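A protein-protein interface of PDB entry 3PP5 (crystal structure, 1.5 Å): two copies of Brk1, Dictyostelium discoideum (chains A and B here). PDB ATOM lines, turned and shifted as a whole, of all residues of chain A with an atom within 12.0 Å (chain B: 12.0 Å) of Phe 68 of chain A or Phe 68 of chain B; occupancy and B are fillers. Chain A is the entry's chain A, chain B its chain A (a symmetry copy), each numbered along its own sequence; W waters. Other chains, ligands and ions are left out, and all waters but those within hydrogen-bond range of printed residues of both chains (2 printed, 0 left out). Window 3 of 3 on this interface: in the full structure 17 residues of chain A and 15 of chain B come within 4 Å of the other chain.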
ATOM      1  N   ARG A  59     -10.139  11.818 -12.039  1.00  0.00           N
ATOM      2  CA  ARG A  59     -10.350  13.269 -12.097  1.00  0.00           C
ATOM      3  C   ARG A  59     -11.468  13.617 -13.085  1.00  0.00           C
ATOM      4  O   ARG A  59     -12.328  14.474 -12.858  1.00  0.00           O
ATOM      5  CB  ARG A  59      -9.076  14.001 -12.480  1.00  0.00           C
ATOM      6  CG  ARG A  59      -7.994  13.962 -11.427  1.00  0.00           C
ATOM      7  CD  ARG A  59      -6.965  15.080 -11.686  1.00  0.00           C
ATOM      8  NE  ARG A  59      -6.039  14.712 -12.747  1.00  0.00           N
ATOM      9  CZ  ARG A  59      -4.847  14.172 -12.523  1.00  0.00           C
ATOM     10  NH1 ARG A  59      -4.439  13.968 -11.277  1.00  0.00           N
ATOM     11  NH2 ARG A  59      -4.059  13.852 -13.537  1.00  0.00           N
ATOM     12  N   GLN A  60     -11.468  12.925 -14.230  1.00  0.00           N
ATOM     13  CA  GLN A  60     -12.491  13.145 -15.241  1.00  0.00           C
ATOM     14  C   GLN A  60     -13.880  12.807 -14.703  1.00  0.00           C
ATOM     15  O   GLN A  60     -14.837  13.554 -14.921  1.00  0.00           O
ATOM     16  CB  GLN A  60     -12.112  12.312 -16.485  1.00  0.00           C
ATOM     17  CG  GLN A  60     -13.012  12.435 -17.639  1.00  0.00           C
ATOM     18  CD  GLN A  60     -12.493  11.676 -18.879  1.00  0.00           C
ATOM     19  OE1 GLN A  60     -11.405  11.070 -18.882  1.00  0.00           O
ATOM     20  NE2 GLN A  60     -13.309  11.682 -19.900  1.00  0.00           N
ATOM     21  N   VAL A  61     -14.006  11.720 -13.947  1.00  0.00           N
ATOM     22  CA  VAL A  61     -15.286  11.333 -13.392  1.00  0.00           C
ATOM     23  C   VAL A  61     -15.738  12.326 -12.321  1.00  0.00           C
ATOM     24  O   VAL A  61     -16.926  12.733 -12.298  1.00  0.00           O
ATOM     25  CB  VAL A  61     -15.196   9.883 -12.794  1.00  0.00           C
ATOM     26  CG1 VAL A  61     -16.414   9.503 -12.016  1.00  0.00           C
ATOM     27  CG2 VAL A  61     -14.996   8.874 -13.933  1.00  0.00           C
ATOM     28  N   ASP A  62     -14.826  12.756 -11.455  1.00  0.00           N
ATOM     29  CA  ASP A  62     -15.207  13.734 -10.426  1.00  0.00           C
ATOM     30  C   ASP A  62     -15.658  15.042 -11.049  1.00  0.00           C
ATOM     31  O   ASP A  62     -16.587  15.669 -10.519  1.00  0.00           O
ATOM     32  CB  ASP A  62     -14.030  13.987  -9.490  1.00  0.00           C
ATOM     33  CG  ASP A  62     -13.991  13.015  -8.296  1.00  0.00           C
ATOM     34  OD1 ASP A  62     -15.022  12.414  -7.914  1.00  0.00           O
ATOM     35  OD2 ASP A  62     -12.900  12.921  -7.725  1.00  0.00           O
ATOM     36  N   TYR A  63     -15.027  15.447 -12.151  1.00  0.00           N
ATOM     37  CA  TYR A  63     -15.447  16.709 -12.789  1.00  0.00           C
ATOM     38  C   TYR A  63     -16.804  16.563 -13.424  1.00  0.00           C
ATOM     39  O   TYR A  63     -17.639  17.492 -13.371  1.00  0.00           O
ATOM     40  CB  TYR A  63     -14.403  17.156 -13.814  1.00  0.00           C
ATOM     41  CG  TYR A  63     -14.682  18.510 -14.441  1.00  0.00           C
ATOM     42  CD1 TYR A  63     -14.359  19.680 -13.775  1.00  0.00           C
ATOM     43  CD2 TYR A  63     -15.248  18.606 -15.700  1.00  0.00           C
ATOM     44  CE1 TYR A  63     -14.605  20.919 -14.345  1.00  0.00           C
ATOM     45  CE2 TYR A  63     -15.501  19.845 -16.285  1.00  0.00           C
ATOM     46  CZ  TYR A  63     -15.178  20.993 -15.599  1.00  0.00           C
ATOM     47  OH  TYR A  63     -15.426  22.225 -16.168  1.00  0.00           O
ATOM     48  N   LEU A  64     -17.073  15.405 -14.024  1.00  0.00           N
ATOM     49  CA  LEU A  64     -18.363  15.165 -14.650  1.00  0.00           C
ATOM     50  C   LEU A  64     -19.446  15.194 -13.578  1.00  0.00           C
ATOM     51  O   LEU A  64     -20.513  15.777 -13.784  1.00  0.00           O
ATOM     52  CB  LEU A  64     -18.287  13.831 -15.419  1.00  0.00           C
ATOM     53  CG  LEU A  64     -19.432  13.371 -16.275  1.00  0.00           C
ATOM     54  CD1 LEU A  64     -19.729  14.397 -17.327  1.00  0.00           C
ATOM     55  CD2 LEU A  64     -18.984  12.058 -16.910  1.00  0.00           C
ATOM     56  N   GLU A  65     -19.179  14.606 -12.411  1.00  0.00           N
ATOM     57  CA  GLU A  65     -20.104  14.619 -11.287  1.00  0.00           C
ATOM     58  C   GLU A  65     -20.434  16.028 -10.904  1.00  0.00           C
ATOM     59  O   GLU A  65     -21.612  16.378 -10.766  1.00  0.00           O
ATOM     60  CB  GLU A  65     -19.520  13.926 -10.037  1.00  0.00           C
ATOM     61  CG  GLU A  65     -19.537  12.418 -10.092  1.00  0.00           C
ATOM     62  CD  GLU A  65     -19.027  11.771  -8.819  1.00  0.00           C
ATOM     63  OE1 GLU A  65     -18.289  12.426  -8.049  1.00  0.00           O
ATOM     64  OE2 GLU A  65     -19.315  10.576  -8.602  1.00  0.00           O
ATOM     65  N   ALA A  66     -19.391  16.833 -10.714  1.00  0.00           N
ATOM     66  CA  ALA A  66     -19.563  18.208 -10.251  1.00  0.00           C
ATOM     67  C   ALA A  66     -20.386  18.994 -11.280  1.00  0.00           C
ATOM     68  O   ALA A  66     -21.261  19.789 -10.904  1.00  0.00           O
ATOM     69  CB  ALA A  66     -18.206  18.866 -10.010  1.00  0.00           C
ATOM     70  N   THR A  67     -20.125  18.769 -12.571  1.00  0.00           N
ATOM     71  CA  THR A  67     -20.853  19.499 -13.633  1.00  0.00           C
ATOM     72  C   THR A  67     -22.309  19.098 -13.694  1.00  0.00           C
ATOM     73  O   THR A  67     -23.193  19.948 -13.936  1.00  0.00           O
ATOM     74  CB  THR A  67     -20.234  19.214 -15.021  1.00  0.00           C
ATOM     75  OG1 THR A  67     -18.852  19.585 -15.017  1.00  0.00           O
ATOM     76  CG2 THR A  67     -20.961  20.016 -16.090  1.00  0.00           C
ATOM     77  N   PHE A  68     -22.587  17.819 -13.488  1.00  0.00           N
ATOM     78  CA  PHE A  68     -23.968  17.343 -13.476  1.00  0.00           C
ATOM     79  C   PHE A  68     -24.743  17.790 -12.244  1.00  0.00           C
ATOM     80  O   PHE A  68     -25.880  18.266 -12.356  1.00  0.00           O
ATOM     81  CB  PHE A  68     -24.032  15.821 -13.575  1.00  0.00           C
ATOM     82  CG  PHE A  68     -25.403  15.271 -13.328  1.00  0.00           C
ATOM     83  CD1 PHE A  68     -26.360  15.284 -14.337  1.00  0.00           C
ATOM     84  CD2 PHE A  68     -25.748  14.766 -12.083  1.00  0.00           C
ATOM     85  CE1 PHE A  68     -27.631  14.785 -14.112  1.00  0.00           C
ATOM     86  CE2 PHE A  68     -27.018  14.270 -11.849  1.00  0.00           C
ATOM     87  CZ  PHE A  68     -27.960  14.277 -12.866  1.00  0.00           C
ATOM     88  N   LYS A  69     -24.140  17.616 -11.069  1.00  0.00           N
ATOM     89  CA  LYS A  69     -24.814  17.914  -9.806  1.00  0.00           C
ATOM     90  C   LYS A  69     -25.118  19.410  -9.661  1.00  0.00           C
ATOM     91  O   LYS A  69     -26.053  19.800  -8.952  1.00  0.00           O
ATOM     92  CB  LYS A  69     -23.995  17.415  -8.608  1.00  0.00           C
ATOM     93  CG  LYS A  69     -23.976  15.888  -8.433  1.00  0.00           C
ATOM     94  CD  LYS A  69     -23.051  15.463  -7.296  1.00  0.00           C
ATOM     95  CE  LYS A  69     -23.356  14.058  -6.775  1.00  0.00           C
ATOM     96  NZ  LYS A  69     -22.450  13.698  -5.620  1.00  0.00           N
ATOM     97  N   THR A  70     -24.332  20.245 -10.333  1.00  0.00           N
ATOM     98  CA  THR A  70     -24.535  21.690 -10.262  1.00  0.00           C
ATOM     99  C   THR A  70     -25.454  22.158 -11.384  1.00  0.00           C
ATOM    100  O   THR A  70     -26.312  21.402 -11.847  1.00  0.00           O
ATOM    101  CB  THR A  70     -23.197  22.461 -10.313  1.00  0.00           C
ATOM    102  OG1 THR A  70     -22.528  22.190 -11.553  1.00  0.00           O
ATOM    103  CG2 THR A  70     -22.293  22.042  -9.148  1.00  0.00           C
ATOM    104  N   ARG B  59     -18.161   1.718  -9.759  1.00  0.00           N
ATOM    105  CA  ARG B  59     -19.436   1.935  -9.064  1.00  0.00           C
ATOM    106  C   ARG B  59     -19.867   3.402  -9.169  1.00  0.00           C
ATOM    107  O   ARG B  59     -21.033   3.749  -9.385  1.00  0.00           O
ATOM    108  CB  ARG B  59     -19.351   1.525  -7.606  1.00  0.00           C
ATOM    109  CG  ARG B  59     -19.213   0.038  -7.383  1.00  0.00           C
ATOM    110  CD  ARG B  59     -19.599  -0.318  -5.933  1.00  0.00           C
ATOM    111  NE  ARG B  59     -18.518  -0.011  -5.007  1.00  0.00           N
ATOM    112  CZ  ARG B  59     -17.627  -0.907  -4.599  1.00  0.00           C
ATOM    113  NH1 ARG B  59     -17.715  -2.163  -5.021  1.00  0.00           N
ATOM    114  NH2 ARG B  59     -16.664  -0.557  -3.764  1.00  0.00           N
ATOM    115  N   GLN B  60     -18.895   4.306  -9.018  1.00  0.00           N
ATOM    116  CA  GLN B  60     -19.171   5.732  -9.118  1.00  0.00           C
ATOM    117  C   GLN B  60     -19.686   6.097 -10.509  1.00  0.00           C
ATOM    118  O   GLN B  60     -20.648   6.857 -10.643  1.00  0.00           O
ATOM    119  CB  GLN B  60     -17.881   6.491  -8.739  1.00  0.00           C
ATOM    120  CG  GLN B  60     -17.973   7.956  -8.744  1.00  0.00           C
ATOM    121  CD  GLN B  60     -16.685   8.633  -8.230  1.00  0.00           C
ATOM    122  OE1 GLN B  60     -15.706   7.979  -7.823  1.00  0.00           O
ATOM    123  NE2 GLN B  60     -16.690   9.938  -8.304  1.00  0.00           N
ATOM    124  N   VAL B  61     -19.105   5.522 -11.558  1.00  0.00           N
ATOM    125  CA  VAL B  61     -19.538   5.808 -12.909  1.00  0.00           C
ATOM    126  C   VAL B  61     -20.932   5.236 -13.167  1.00  0.00           C
ATOM    127  O   VAL B  61     -21.797   5.926 -13.762  1.00  0.00           O
ATOM    128  CB  VAL B  61     -18.506   5.223 -13.940  1.00  0.00           C
ATOM    129  CG1 VAL B  61     -18.995   5.291 -15.349  1.00  0.00           C
ATOM    130  CG2 VAL B  61     -17.184   5.996 -13.831  1.00  0.00           C
ATOM    131  N   ASP B  62     -21.192   4.015 -12.711  1.00  0.00           N
ATOM    132  CA  ASP B  62     -22.528   3.437 -12.909  1.00  0.00           C
ATOM    133  C   ASP B  62     -23.592   4.248 -12.194  1.00  0.00           C
ATOM    134  O   ASP B  62     -24.703   4.382 -12.726  1.00  0.00           O
ATOM    135  CB  ASP B  62     -22.550   1.997 -12.403  1.00  0.00           C
ATOM    136  CG  ASP B  62     -22.145   0.975 -13.481  1.00  0.00           C
ATOM    137  OD1 ASP B  62     -22.231   1.249 -14.701  1.00  0.00           O
ATOM    138  OD2 ASP B  62     -21.789  -0.129 -13.057  1.00  0.00           O
ATOM    139  N   TYR B  63     -23.267   4.786 -11.018  1.00  0.00           N
ATOM    140  CA  TYR B  63     -24.274   5.589 -10.299  1.00  0.00           C
ATOM    141  C   TYR B  63     -24.524   6.894 -11.010  1.00  0.00           C
ATOM    142  O   TYR B  63     -25.678   7.369 -11.086  1.00  0.00           O
ATOM    143  CB  TYR B  63     -23.830   5.825  -8.855  1.00  0.00           C
ATOM    144  CG  TYR B  63     -24.855   6.541  -7.994  1.00  0.00           C
ATOM    145  CD1 TYR B  63     -25.916   5.850  -7.433  1.00  0.00           C
ATOM    146  CD2 TYR B  63     -24.743   7.895  -7.734  1.00  0.00           C
ATOM    147  CE1 TYR B  63     -26.851   6.497  -6.640  1.00  0.00           C
ATOM    148  CE2 TYR B  63     -25.676   8.558  -6.941  1.00  0.00           C
ATOM    149  CZ  TYR B  63     -26.726   7.850  -6.400  1.00  0.00           C
ATOM    150  OH  TYR B  63     -27.657   8.497  -5.615  1.00  0.00           O
ATOM    151  N   LEU B  64     -23.473   7.499 -11.558  1.00  0.00           N
ATOM    152  CA  LEU B  64     -23.621   8.752 -12.279  1.00  0.00           C
ATOM    153  C   LEU B  64     -24.492   8.518 -13.506  1.00  0.00           C
ATOM    154  O   LEU B  64     -25.370   9.328 -13.813  1.00  0.00           O
ATOM    155  CB  LEU B  64     -22.213   9.287 -12.612  1.00  0.00           C
ATOM    156  CG  LEU B  64     -22.034  10.636 -13.247  1.00  0.00           C
ATOM    157  CD1 LEU B  64     -22.647  11.695 -12.383  1.00  0.00           C
ATOM    158  CD2 LEU B  64     -20.528  10.845 -13.376  1.00  0.00           C
ATOM    159  N   GLU B  65     -24.295   7.396 -14.202  1.00  0.00           N
ATOM    160  CA  GLU B  65     -25.103   7.027 -15.355  1.00  0.00           C
ATOM    161  C   GLU B  65     -26.549   6.956 -14.974  1.00  0.00           C
ATOM    162  O   GLU B  65     -27.403   7.544 -15.647  1.00  0.00           O
ATOM    163  CB  GLU B  65     -24.710   5.649 -15.931  1.00  0.00           C
ATOM    164  CG  GLU B  65     -23.449   5.655 -16.759  1.00  0.00           C
ATOM    165  CD  GLU B  65     -23.133   4.303 -17.371  1.00  0.00           C
ATOM    166  OE1 GLU B  65     -23.622   3.269 -16.863  1.00  0.00           O
ATOM    167  OE2 GLU B  65     -22.345   4.256 -18.337  1.00  0.00           O
ATOM    168  N   ALA B  66     -26.826   6.218 -13.901  1.00  0.00           N
ATOM    169  CA  ALA B  66     -28.202   5.988 -13.467  1.00  0.00           C
ATOM    170  C   ALA B  66     -28.855   7.329 -13.107  1.00  0.00           C
ATOM    171  O   ALA B  66     -30.027   7.563 -13.437  1.00  0.00           O
ATOM    172  CB  ALA B  66     -28.239   5.021 -12.286  1.00  0.00           C
ATOM    173  N   THR B  67     -28.104   8.216 -12.447  1.00  0.00           N
ATOM    174  CA  THR B  67     -28.656   9.526 -12.036  1.00  0.00           C
ATOM    175  C   THR B  67     -28.940  10.414 -13.228  1.00  0.00           C
ATOM    176  O   THR B  67     -29.946  11.155 -13.243  1.00  0.00           O
ATOM    177  CB  THR B  67     -27.664  10.280 -11.121  1.00  0.00           C
ATOM    178  OG1 THR B  67     -27.369   9.481  -9.972  1.00  0.00           O
ATOM    179  CG2 THR B  67     -28.274  11.598 -10.667  1.00  0.00           C
ATOM    180  N   PHE B  68     -28.073  10.367 -14.229  1.00  0.00           N
ATOM    181  CA  PHE B  68     -28.287  11.149 -15.443  1.00  0.00           C
ATOM    182  C   PHE B  68     -29.426  10.619 -16.303  1.00  0.00           C
ATOM    183  O   PHE B  68     -30.279  11.390 -16.761  1.00  0.00           O
ATOM    184  CB  PHE B  68     -27.019  11.218 -16.291  1.00  0.00           C
ATOM    185  CG  PHE B  68     -27.249  11.801 -17.651  1.00  0.00           C
ATOM    186  CD1 PHE B  68     -27.326  13.179 -17.823  1.00  0.00           C
ATOM    187  CD2 PHE B  68     -27.416  10.976 -18.754  1.00  0.00           C
ATOM    188  CE1 PHE B  68     -27.547  13.723 -19.076  1.00  0.00           C
ATOM    189  CE2 PHE B  68     -27.642  11.514 -20.009  1.00  0.00           C
ATOM    190  CZ  PHE B  68     -27.705  12.889 -20.171  1.00  0.00           C
ATOM    191  N   LYS B  69     -29.429   9.308 -16.541  1.00  0.00           N
ATOM    192  CA  LYS B  69     -30.411   8.688 -17.428  1.00  0.00           C
ATOM    193  C   LYS B  69     -31.835   8.798 -16.869  1.00  0.00           C
ATOM    194  O   LYS B  69     -32.814   8.783 -17.623  1.00  0.00           O
ATOM    195  CB  LYS B  69     -30.058   7.222 -17.712  1.00  0.00           C
ATOM    196  CG  LYS B  69     -28.845   7.019 -18.633  1.00  0.00           C
ATOM    197  CD  LYS B  69     -28.485   5.542 -18.774  1.00  0.00           C
ATOM    198  CE  LYS B  69     -27.635   5.252 -20.012  1.00  0.00           C
ATOM    199  NZ  LYS B  69     -27.344   3.775 -20.137  1.00  0.00           N
ATOM    200  N   THR B  70     -31.948   8.911 -15.549  1.00  0.00           N
ATOM    201  CA  THR B  70     -33.260   9.019 -14.915  1.00  0.00           C
ATOM    202  C   THR B  70     -33.658  10.481 -14.752  1.00  0.00           C
ATOM    203  O   THR B  70     -33.244  11.334 -15.544  1.00  0.00           O
ATOM    204  CB  THR B  70     -33.295   8.304 -13.546  1.00  0.00           C
ATOM    205  OG1 THR B  70     -32.345   8.908 -12.657  1.00  0.00           O
ATOM    206  CG2 THR B  70     -32.959   6.816 -13.709  1.00  0.00           C
HETATM  207  O   HOH W   1     -21.444   8.949  -8.871  1.00  0.00           O
HETATM  208  O   HOH W   2     -13.490   9.596  -7.128  1.00  0.00           O
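Phe 68 of chain B touches just one residue of chain A: Phe 68.
No residue of chain B comes within 4 Å of Lys 69 of chain A.
No residue of chain A comes within 4 Å of Ala 66 of chain B.
No residue of chain A comes within 4 Å of Lys 69 of chain B.
No residue of chain A comes within 4 Å of Thr 70 of chain B.
Printed residues of chain B within 4 Å of Val 61 of chain A: Gln 60 (3.7 Å) and Val 61 (3.6 Å).
Of the printed residues of chain A, Val 61 of chain B touches Val 61 (3.6 Å).
Printed residues of chain B within 4 Å of Leu 64 of chain A: Leu 64 (3.998 Å).
Printed residues of chain A within 4 Å of Gln 60 of chain B: Val 61 (3.7 Å), Asp 62 (3.0 Å) and Glu 65 (2.7 Å).
Tyr 63 of chain A touches none of the printed residues of chain B.
The nearest residue of chain B that does not touch Phe 68 of chain A is Leu 64 of chain B (4.4 Å).
The nearest residue of chain A that does not touch Phe 68 of chain B is Leu 64 of chain A (7.7 Å).
Val 61 of chain A touches its own counterpart, Val 61 of chain B.
Leu 64 of chain A touches its own counterpart, Leu 64 of chain B.
Glu 65 of chain A touches Gln 60 of chain B, but with the chains exchanged Gln 60 of chain A does not touch Glu 65 of chain B (11.3 Å).
Phe 68 of chain A touches its own counterpart, Phe 68 of chain B.
Positions printed for both chains: 59, 60, 61, 62, 63, 64, 65, 66, 67, 68, 69 and 70.
Of the 8 pairs that touch across the chains among the printed residues, 3 have their exchanged pair printed and touching as well.
Among the printed residues, merely in contact across the chains: Phe 68 of chain A with Thr 67 of chain B, Val 61 of chain A with Val 61 of chain B, Val 61 of chain A with Gln 60 of chain B, Glu 65 of chain A with Leu 64 of chain B, Phe 68 of chain A with Phe 68 of chain B and Leu 64 of chain A with Leu 64 of chain B.
Water W1 bridges the side-chain carboxylate of Glu 65 of chain A and the backbone carbonyl oxygen of Gln 60 of chain B.
Water W2 lies within hydrogen-bond range of OE1 of Gln 60 of chain B (2.8 Å) and OD1 of Asp 62 of chain A (3.3 Å).
Of the 12 printed residues of chain A, 5 touch a printed residue of chain B.
Printed residues of chain A that touch a printed residue of chain B: Val 61, Asp 62, Leu 64, Glu 65 and Phe 68.
Of the 12 printed residues of chain B, 5 touch a printed residue of chain A.
Among the printed residues, 8 pairs touch across the chains.
Among the printed residues, no Asp or Glu carboxylate lies within 4 Å of a Lys or Arg side-chain nitrogen of the other chain.
NE2 of Gln 60 of chain B is in hydrogen-bond range of OD1 of Asp 62 of chain A (3.0 Å).
The side-chain amide nitrogen (NE2) of Gln 60 of chain B is in hydrogen-bond range of the side-chain carboxylate (OE2) of Glu 65 of chain A (2.7 Å).
O of Thr 67 of chain B sits at hydrogen-bond distance from OG1 of Thr 70 of chain B (3.3 Å).
O of Tyr 63 of chain B lies within hydrogen-bond range of OG1 of Thr 67 of chain B, at 2.9 Å.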
